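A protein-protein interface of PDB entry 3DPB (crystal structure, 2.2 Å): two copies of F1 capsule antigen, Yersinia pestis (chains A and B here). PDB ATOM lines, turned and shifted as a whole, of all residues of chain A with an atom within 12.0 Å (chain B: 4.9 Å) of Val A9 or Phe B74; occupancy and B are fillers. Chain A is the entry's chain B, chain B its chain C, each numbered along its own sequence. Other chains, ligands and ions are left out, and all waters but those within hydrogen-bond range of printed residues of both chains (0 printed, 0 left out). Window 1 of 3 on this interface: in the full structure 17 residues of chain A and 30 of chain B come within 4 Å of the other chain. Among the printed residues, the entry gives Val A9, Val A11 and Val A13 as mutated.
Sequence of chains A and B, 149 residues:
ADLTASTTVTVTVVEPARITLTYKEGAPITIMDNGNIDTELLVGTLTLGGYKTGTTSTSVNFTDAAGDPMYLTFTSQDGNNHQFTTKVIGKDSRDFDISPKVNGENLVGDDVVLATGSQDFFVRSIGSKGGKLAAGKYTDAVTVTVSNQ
No position is printed for both chains. Of the 17 pairs that touch across the chains among the printed residues, none has its exchanged pair printed and touching as well.
Among the printed residues, pairs that only touch across the chains: Ser A6 with Val B142, Val A9 with Thr B139, Val A9 with Tyr B23, Thr A10 with Thr B139, Thr A10 with Tyr B138, Val A11 with Phe B74, Val A13 with Tyr B138, Thr A8 with Asp B140, Val A9 with Phe B74, Val A13 with Phe B84, Val A11 with Phe B84, Val A9 with Tyr B138, Val A9 with Val B142 and Thr A7 with Asp B140.
Hydrophobic or aromatic side chains of chain A that line the printed part of chain B: Val A9, Val A11 and Val A13. Hydrophobic or aromatic side chains of chain B within 4 Å of the printed part of chain A: Tyr B23, Phe B74, Phe B84, Tyr B138 and Val B142.
The backbone carbonyl oxygen (O) of Thr A7 lies within hydrogen-bond range of the backbone NH (N) of Val B142 (2.7 Å). The backbone NH of Val A9 lies within hydrogen-bond range of the backbone carbonyl oxygen of Asp B140, 2.9 Å away. The backbone NH of Tyr B138 sits at hydrogen-bond distance from the backbone carbonyl oxygen of Val A11 (2.8 Å).
The backbone NH (N) of Phe B74 lies within hydrogen-bond range of the backbone carbonyl oxygen (O) of Phe B84, 2.8 Å away. The backbone carbonyl oxygen (O) of Thr B75 sits at hydrogen-bond distance from the backbone NH (N) of Thr B139.
Val A9 touches just these residues of chain B: Tyr B23, Phe B74, Tyr B138, Thr B139, Asp B140 and Val B142. Of chain A, only Val A9 and Val A11 come within 4 Å of Phe B74. Tyr B23 touches just one residue of chain A: Val A9. No residue of chain A comes within 4 Å of Leu B72. No residue of chain A comes within 4 Å of Thr B73. No residue of chain A comes within 4 Å of Thr B75. No residue of chain A comes within 4 Å of Ser B76. Of chain A, only Val A11 and Val A13 come within 4 Å of Phe B84. No residue of chain A comes within 4 Å of Thr B86. Tyr B138 touches just these residues of chain A: Val A9 (3.9 Å), Thr A10 (3.4 Å), Val A11 (2.8 Å) and Val A13 (3.6 Å). Thr B139 touches just these residues of chain A: Val A9 (3.3 Å) and Thr A10 (3.4 Å). Printed residues of chain A within 4 Å of Asp B140: Thr A7 (3.9 Å), Thr A8 (3.6 Å) and Val A9 (2.9 Å). Val B142 touches just these residues of chain A: Ser A6, Thr A7 and Val A9. Printed residues of chain B within 4 Å of Thr A10: Tyr B138 (3.4 Å) and Thr B139 (3.4 Å). Of the printed residues of chain B, Ser A6 touches Val B142. Of the printed residues of chain B, Thr A8 touches Asp B140. The nearest residue of chain B that does not touch Val A9 is Leu B46 (4.2 Å). The nearest residue of chain A that does not touch Phe B74 is Thr A10 (5.1 Å). The nearest printed residue of chain B that does not touch Thr A8 is Thr B139 (4.6 Å).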
ATOM      1  N   ALA A   5      22.115 -18.876  -7.348  1.00  0.00           N
ATOM      2  CA  ALA A   5      21.597 -19.362  -6.088  1.00  0.00           C
ATOM      3  C   ALA A   5      20.099 -19.670  -6.330  1.00  0.00           C
ATOM      4  O   ALA A   5      19.546 -19.293  -7.369  1.00  0.00           O
ATOM      5  CB  ALA A   5      21.769 -18.308  -5.018  1.00  0.00           C
ATOM      6  N   SER A   6      19.441 -20.347  -5.397  1.00  0.00           N
ATOM      7  CA  SER A   6      18.027 -20.653  -5.587  1.00  0.00           C
ATOM      8  C   SER A   6      17.260 -20.741  -4.265  1.00  0.00           C
ATOM      9  O   SER A   6      17.817 -21.080  -3.209  1.00  0.00           O
ATOM     10  CB  SER A   6      17.876 -21.920  -6.428  1.00  0.00           C
ATOM     11  OG  SER A   6      18.111 -23.036  -5.606  1.00  0.00           O
ATOM     12  N   THR A   7      15.990 -20.363  -4.310  1.00  0.00           N
ATOM     13  CA  THR A   7      15.133 -20.452  -3.133  1.00  0.00           C
ATOM     14  C   THR A   7      13.710 -20.862  -3.522  1.00  0.00           C
ATOM     15  O   THR A   7      13.307 -20.689  -4.659  1.00  0.00           O
ATOM     16  CB  THR A   7      15.215 -19.164  -2.252  1.00  0.00           C
ATOM     17  OG1 THR A   7      14.862 -19.492  -0.901  1.00  0.00           O
ATOM     18  CG2 THR A   7      14.363 -18.029  -2.784  1.00  0.00           C
ATOM     19  N   THR A   8      12.996 -21.467  -2.584  1.00  0.00           N
ATOM     20  CA  THR A   8      11.620 -21.851  -2.784  1.00  0.00           C
ATOM     21  C   THR A   8      10.788 -20.816  -2.034  1.00  0.00           C
ATOM     22  O   THR A   8      10.965 -20.643  -0.845  1.00  0.00           O
ATOM     23  CB  THR A   8      11.357 -23.322  -2.326  1.00  0.00           C
ATOM     24  OG1 THR A   8      12.188 -24.204  -3.092  1.00  0.00           O
ATOM     25  CG2 THR A   8       9.914 -23.756  -2.545  1.00  0.00           C
ATOM     26  N   VAL A   9       9.942 -20.100  -2.770  1.00  0.00           N
ATOM     27  CA  VAL A   9       9.084 -19.034  -2.238  1.00  0.00           C
ATOM     28  C   VAL A   9       7.663 -19.547  -2.042  1.00  0.00           C
ATOM     29  O   VAL A   9       7.058 -20.057  -2.980  1.00  0.00           O
ATOM     30  CB  VAL A   9       9.030 -17.859  -3.198  1.00  0.00           C
ATOM     31  CG1 VAL A   9       8.120 -16.787  -2.645  1.00  0.00           C
ATOM     32  CG2 VAL A   9      10.428 -17.299  -3.462  1.00  0.00           C
ATOM     33  N   THR A  10       7.152 -19.445  -0.821  1.00  0.00           N
ATOM     34  CA  THR A  10       5.783 -19.889  -0.518  1.00  0.00           C
ATOM     35  C   THR A  10       4.889 -18.685  -0.155  1.00  0.00           C
ATOM     36  O   THR A  10       5.312 -17.790   0.536  1.00  0.00           O
ATOM     37  CB  THR A  10       5.774 -20.956   0.603  1.00  0.00           C
ATOM     38  OG1 THR A  10       6.615 -22.051   0.209  1.00  0.00           O
ATOM     39  CG2 THR A  10       4.351 -21.492   0.841  1.00  0.00           C
ATOM     40  N   VAL A  11       3.664 -18.675  -0.659  1.00  0.00           N
ATOM     41  CA  VAL A  11       2.750 -17.536  -0.531  1.00  0.00           C
ATOM     42  C   VAL A  11       1.433 -18.089   0.002  1.00  0.00           C
ATOM     43  O   VAL A  11       0.954 -19.133  -0.469  1.00  0.00           O
ATOM     44  CB  VAL A  11       2.516 -16.826  -1.910  1.00  0.00           C
ATOM     45  CG1 VAL A  11       1.549 -15.666  -1.792  1.00  0.00           C
ATOM     46  CG2 VAL A  11       3.835 -16.298  -2.490  1.00  0.00           C
ATOM     47  N   THR A  12       0.876 -17.418   1.003  1.00  0.00           N
ATOM     48  CA  THR A  12      -0.396 -17.805   1.606  1.00  0.00           C
ATOM     49  C   THR A  12      -1.504 -16.954   0.962  1.00  0.00           C
ATOM     50  O   THR A  12      -1.458 -15.736   0.979  1.00  0.00           O
ATOM     51  CB  THR A  12      -0.375 -17.554   3.128  1.00  0.00           C
ATOM     52  OG1 THR A  12       0.691 -18.288   3.711  1.00  0.00           O
ATOM     53  CG2 THR A  12      -1.710 -17.947   3.802  1.00  0.00           C
ATOM     54  N   VAL A  13      -2.466 -17.611   0.358  1.00  0.00           N
ATOM     55  CA  VAL A  13      -3.549 -16.943  -0.299  1.00  0.00           C
ATOM     56  C   VAL A  13      -4.822 -17.286   0.523  1.00  0.00           C
ATOM     57  O   VAL A  13      -5.114 -18.476   0.732  1.00  0.00           O
ATOM     58  CB  VAL A  13      -3.660 -17.383  -1.771  1.00  0.00           C
ATOM     59  CG1 VAL A  13      -4.817 -16.661  -2.463  1.00  0.00           C
ATOM     60  CG2 VAL A  13      -2.319 -17.100  -2.529  1.00  0.00           C
ATOM     61  N   VAL A  14      -5.528 -16.270   1.015  1.00  0.00           N
ATOM     62  CA  VAL A  14      -6.669 -16.508   1.905  1.00  0.00           C
ATOM     63  C   VAL A  14      -7.997 -16.044   1.328  1.00  0.00           C
ATOM     64  O   VAL A  14      -8.077 -15.071   0.594  1.00  0.00           O
ATOM     65  CB  VAL A  14      -6.477 -15.920   3.347  1.00  0.00           C
ATOM     66  CG1 VAL A  14      -5.156 -16.361   3.944  1.00  0.00           C
ATOM     67  CG2 VAL A  14      -6.590 -14.411   3.351  1.00  0.00           C
ATOM     68  N   TYR B  23      14.423 -15.095   1.124  1.00  0.00           N
ATOM     69  CA  TYR B  23      13.086 -14.588   0.937  1.00  0.00           C
ATOM     70  C   TYR B  23      12.376 -14.388   2.268  1.00  0.00           C
ATOM     71  O   TYR B  23      12.404 -15.259   3.133  1.00  0.00           O
ATOM     72  CB  TYR B  23      12.272 -15.550   0.062  1.00  0.00           C
ATOM     73  CG  TYR B  23      10.833 -15.117  -0.125  1.00  0.00           C
ATOM     74  CD1 TYR B  23      10.504 -14.115  -1.053  1.00  0.00           C
ATOM     75  CD2 TYR B  23       9.801 -15.706   0.623  1.00  0.00           C
ATOM     76  CE1 TYR B  23       9.193 -13.704  -1.231  1.00  0.00           C
ATOM     77  CE2 TYR B  23       8.468 -15.299   0.446  1.00  0.00           C
ATOM     78  CZ  TYR B  23       8.181 -14.291  -0.486  1.00  0.00           C
ATOM     79  OH  TYR B  23       6.894 -13.865  -0.701  1.00  0.00           O
ATOM     80  N   LEU B  46      12.676 -10.531  -1.891  1.00  0.00           N
ATOM     81  CA  LEU B  46      13.852 -11.326  -2.197  1.00  0.00           C
ATOM     82  C   LEU B  46      15.078 -10.501  -1.880  1.00  0.00           C
ATOM     83  O   LEU B  46      15.161  -9.343  -2.268  1.00  0.00           O
ATOM     84  CB  LEU B  46      13.870 -11.735  -3.670  1.00  0.00           C
ATOM     85  CG  LEU B  46      12.849 -12.767  -4.157  1.00  0.00           C
ATOM     86  CD1 LEU B  46      12.737 -12.639  -5.665  1.00  0.00           C
ATOM     87  CD2 LEU B  46      13.237 -14.228  -3.728  1.00  0.00           C
ATOM     88  N   LEU B  72       7.278 -13.996 -12.525  1.00  0.00           N
ATOM     89  CA  LEU B  72       7.343 -15.198 -11.715  1.00  0.00           C
ATOM     90  C   LEU B  72       5.921 -15.764 -11.519  1.00  0.00           C
ATOM     91  O   LEU B  72       4.972 -15.022 -11.239  1.00  0.00           O
ATOM     92  CB  LEU B  72       8.027 -14.925 -10.371  1.00  0.00           C
ATOM     93  CG  LEU B  72       9.550 -14.619 -10.352  1.00  0.00           C
ATOM     94  CD1 LEU B  72      10.097 -14.585  -8.875  1.00  0.00           C
ATOM     95  CD2 LEU B  72      10.340 -15.644 -11.175  1.00  0.00           C
ATOM     96  N   THR B  73       5.791 -17.075 -11.658  1.00  0.00           N
ATOM     97  CA  THR B  73       4.519 -17.761 -11.692  1.00  0.00           C
ATOM     98  C   THR B  73       4.350 -18.669 -10.487  1.00  0.00           C
ATOM     99  O   THR B  73       5.206 -19.522 -10.231  1.00  0.00           O
ATOM    100  CB  THR B  73       4.392 -18.606 -12.952  1.00  0.00           C
ATOM    101  OG1 THR B  73       4.464 -17.736 -14.068  1.00  0.00           O
ATOM    102  CG2 THR B  73       3.028 -19.321 -13.024  1.00  0.00           C
ATOM    103  N   PHE B  74       3.239 -18.475  -9.768  1.00  0.00           N
ATOM    104  CA  PHE B  74       2.934 -19.222  -8.556  1.00  0.00           C
ATOM    105  C   PHE B  74       1.789 -20.158  -8.793  1.00  0.00           C
ATOM    106  O   PHE B  74       0.785 -19.792  -9.395  1.00  0.00           O
ATOM    107  CB  PHE B  74       2.654 -18.305  -7.382  1.00  0.00           C
ATOM    108  CG  PHE B  74       3.874 -17.590  -6.871  1.00  0.00           C
ATOM    109  CD1 PHE B  74       4.359 -16.470  -7.520  1.00  0.00           C
ATOM    110  CD2 PHE B  74       4.523 -18.036  -5.746  1.00  0.00           C
ATOM    111  CE1 PHE B  74       5.529 -15.803  -7.078  1.00  0.00           C
ATOM    112  CE2 PHE B  74       5.679 -17.378  -5.278  1.00  0.00           C
ATOM    113  CZ  PHE B  74       6.181 -16.252  -5.953  1.00  0.00           C
ATOM    114  N   THR B  75       1.947 -21.368  -8.272  1.00  0.00           N
ATOM    115  CA  THR B  75       1.046 -22.457  -8.544  1.00  0.00           C
ATOM    116  C   THR B  75       0.559 -23.087  -7.219  1.00  0.00           C
ATOM    117  O   THR B  75       1.351 -23.230  -6.268  1.00  0.00           O
ATOM    118  CB  THR B  75       1.789 -23.480  -9.399  1.00  0.00           C
ATOM    119  OG1 THR B  75       2.583 -22.794 -10.398  1.00  0.00           O
ATOM    120  CG2 THR B  75       0.781 -24.475 -10.081  1.00  0.00           C
ATOM    121  N   SER B  76      -0.736 -23.415  -7.147  1.00  0.00           N
ATOM    122  CA  SER B  76      -1.330 -24.093  -5.990  1.00  0.00           C
ATOM    123  C   SER B  76      -0.831 -25.539  -5.844  1.00  0.00           C
ATOM    124  O   SER B  76      -0.308 -26.118  -6.810  1.00  0.00           O
ATOM    125  CB  SER B  76      -2.864 -24.076  -6.072  1.00  0.00           C
ATOM    126  OG  SER B  76      -3.348 -24.754  -7.209  1.00  0.00           O
ATOM    127  N   HIS B  82      -4.001 -23.913 -10.016  1.00  0.00           N
ATOM    128  CA  HIS B  82      -4.313 -22.481 -10.035  1.00  0.00           C
ATOM    129  C   HIS B  82      -2.996 -21.778 -10.031  1.00  0.00           C
ATOM    130  O   HIS B  82      -2.077 -22.215  -9.346  1.00  0.00           O
ATOM    131  CB  HIS B  82      -5.163 -22.034  -8.836  1.00  0.00           C
ATOM    132  CG  HIS B  82      -6.477 -22.748  -8.731  1.00  0.00           C
ATOM    133  ND1 HIS B  82      -7.429 -22.706  -9.730  1.00  0.00           N
ATOM    134  CD2 HIS B  82      -6.981 -23.550  -7.760  1.00  0.00           C
ATOM    135  CE1 HIS B  82      -8.465 -23.451  -9.382  1.00  0.00           C
ATOM    136  NE2 HIS B  82      -8.216 -23.980  -8.194  1.00  0.00           N
ATOM    137  N   GLN B  83      -2.905 -20.685 -10.773  1.00  0.00           N
ATOM    138  CA  GLN B  83      -1.687 -19.902 -10.856  1.00  0.00           C
ATOM    139  C   GLN B  83      -1.947 -18.396 -10.839  1.00  0.00           C
ATOM    140  O   GLN B  83      -2.973 -17.903 -11.337  1.00  0.00           O
ATOM    141  CB  GLN B  83      -0.905 -20.287 -12.132  1.00  0.00           C
ATOM    142  CG  GLN B  83      -0.463 -21.756 -12.240  1.00  0.00           C
ATOM    143  CD  GLN B  83       0.383 -22.047 -13.474  1.00  0.00           C
ATOM    144  OE1 GLN B  83      -0.090 -21.939 -14.598  1.00  0.00           O
ATOM    145  NE2 GLN B  83       1.640 -22.459 -13.262  1.00  0.00           N
ATOM    146  N   PHE B  84      -1.006 -17.652 -10.274  1.00  0.00           N
ATOM    147  CA  PHE B  84      -1.027 -16.200 -10.412  1.00  0.00           C
ATOM    148  C   PHE B  84       0.383 -15.779 -10.746  1.00  0.00           C
ATOM    149  O   PHE B  84       1.308 -16.524 -10.451  1.00  0.00           O
ATOM    150  CB  PHE B  84      -1.596 -15.498  -9.128  1.00  0.00           C
ATOM    151  CG  PHE B  84      -0.782 -15.717  -7.867  1.00  0.00           C
ATOM    152  CD1 PHE B  84       0.268 -14.885  -7.550  1.00  0.00           C
ATOM    153  CD2 PHE B  84      -1.116 -16.715  -6.968  1.00  0.00           C
ATOM    154  CE1 PHE B  84       1.000 -15.038  -6.367  1.00  0.00           C
ATOM    155  CE2 PHE B  84      -0.414 -16.866  -5.765  1.00  0.00           C
ATOM    156  CZ  PHE B  84       0.663 -16.034  -5.479  1.00  0.00           C
ATOM    157  N   THR B  86       3.429 -12.591 -10.781  1.00  0.00           N
ATOM    158  CA  THR B  86       3.985 -11.516  -9.983  1.00  0.00           C
ATOM    159  C   THR B  86       5.119 -10.904 -10.782  1.00  0.00           C
ATOM    160  O   THR B  86       5.602 -11.517 -11.717  1.00  0.00           O
ATOM    161  CB  THR B  86       4.547 -11.988  -8.611  1.00  0.00           C
ATOM    162  OG1 THR B  86       5.675 -12.841  -8.801  1.00  0.00           O
ATOM    163  CG2 THR B  86       3.493 -12.686  -7.744  1.00  0.00           C
ATOM    164  N   VAL B 123       8.591  -8.784  -4.555  1.00  0.00           N
ATOM    165  CA  VAL B 123       7.661  -9.576  -5.354  1.00  0.00           C
ATOM    166  C   VAL B 123       6.297  -8.890  -5.228  1.00  0.00           C
ATOM    167  O   VAL B 123       5.775  -8.738  -4.142  1.00  0.00           O
ATOM    168  CB  VAL B 123       7.665 -11.038  -4.880  1.00  0.00           C
ATOM    169  CG1 VAL B 123       6.726 -11.885  -5.705  1.00  0.00           C
ATOM    170  CG2 VAL B 123       9.082 -11.595  -4.995  1.00  0.00           C
ATOM    171  N   TYR B 138       0.723 -21.317  -2.241  1.00  0.00           N
ATOM    172  CA  TYR B 138       1.208 -21.369  -3.601  1.00  0.00           C
ATOM    173  C   TYR B 138       2.712 -21.338  -3.513  1.00  0.00           C
ATOM    174  O   TYR B 138       3.254 -20.663  -2.666  1.00  0.00           O
ATOM    175  CB  TYR B 138       0.668 -20.197  -4.431  1.00  0.00           C
ATOM    176  CG  TYR B 138      -0.800 -20.322  -4.835  1.00  0.00           C
ATOM    177  CD1 TYR B 138      -1.798 -20.366  -3.871  1.00  0.00           C
ATOM    178  CD2 TYR B 138      -1.182 -20.307  -6.172  1.00  0.00           C
ATOM    179  CE1 TYR B 138      -3.118 -20.488  -4.214  1.00  0.00           C
ATOM    180  CE2 TYR B 138      -2.553 -20.388  -6.541  1.00  0.00           C
ATOM    181  CZ  TYR B 138      -3.504 -20.478  -5.546  1.00  0.00           C
ATOM    182  OH  TYR B 138      -4.865 -20.547  -5.849  1.00  0.00           O
ATOM    183  N   THR B 139       3.391 -22.111  -4.358  1.00  0.00           N
ATOM    184  CA  THR B 139       4.869 -22.072  -4.356  1.00  0.00           C
ATOM    185  C   THR B 139       5.425 -21.686  -5.706  1.00  0.00           C
ATOM    186  O   THR B 139       4.735 -21.753  -6.734  1.00  0.00           O
ATOM    187  CB  THR B 139       5.511 -23.396  -3.896  1.00  0.00           C
ATOM    188  OG1 THR B 139       4.947 -24.454  -4.652  1.00  0.00           O
ATOM    189  CG2 THR B 139       5.210 -23.672  -2.413  1.00  0.00           C
ATOM    190  N   ASP B 140       6.679 -21.240  -5.666  1.00  0.00           N
ATOM    191  CA  ASP B 140       7.530 -21.131  -6.848  1.00  0.00           C
ATOM    192  C   ASP B 140       8.967 -21.430  -6.459  1.00  0.00           C
ATOM    193  O   ASP B 140       9.461 -20.875  -5.490  1.00  0.00           O
ATOM    194  CB  ASP B 140       7.461 -19.719  -7.435  1.00  0.00           C
ATOM    195  CG  ASP B 140       7.924 -19.684  -8.865  1.00  0.00           C
ATOM    196  OD1 ASP B 140       7.954 -20.789  -9.483  1.00  0.00           O
ATOM    197  OD2 ASP B 140       8.245 -18.574  -9.371  1.00  0.00           O
ATOM    198  N   VAL B 142      12.449 -20.697  -7.204  1.00  0.00           N
ATOM    199  CA  VAL B 142      13.102 -19.585  -7.896  1.00  0.00           C
ATOM    200  C   VAL B 142      14.616 -19.736  -7.981  1.00  0.00           C
ATOM    201  O   VAL B 142      15.270 -20.075  -6.991  1.00  0.00           O
ATOM    202  CB  VAL B 142      12.744 -18.224  -7.218  1.00  0.00           C
ATOM    203  CG1 VAL B 142      13.400 -17.035  -7.954  1.00  0.00           C
ATOM    204  CG2 VAL B 142      11.219 -18.028  -7.204  1.00  0.00           C
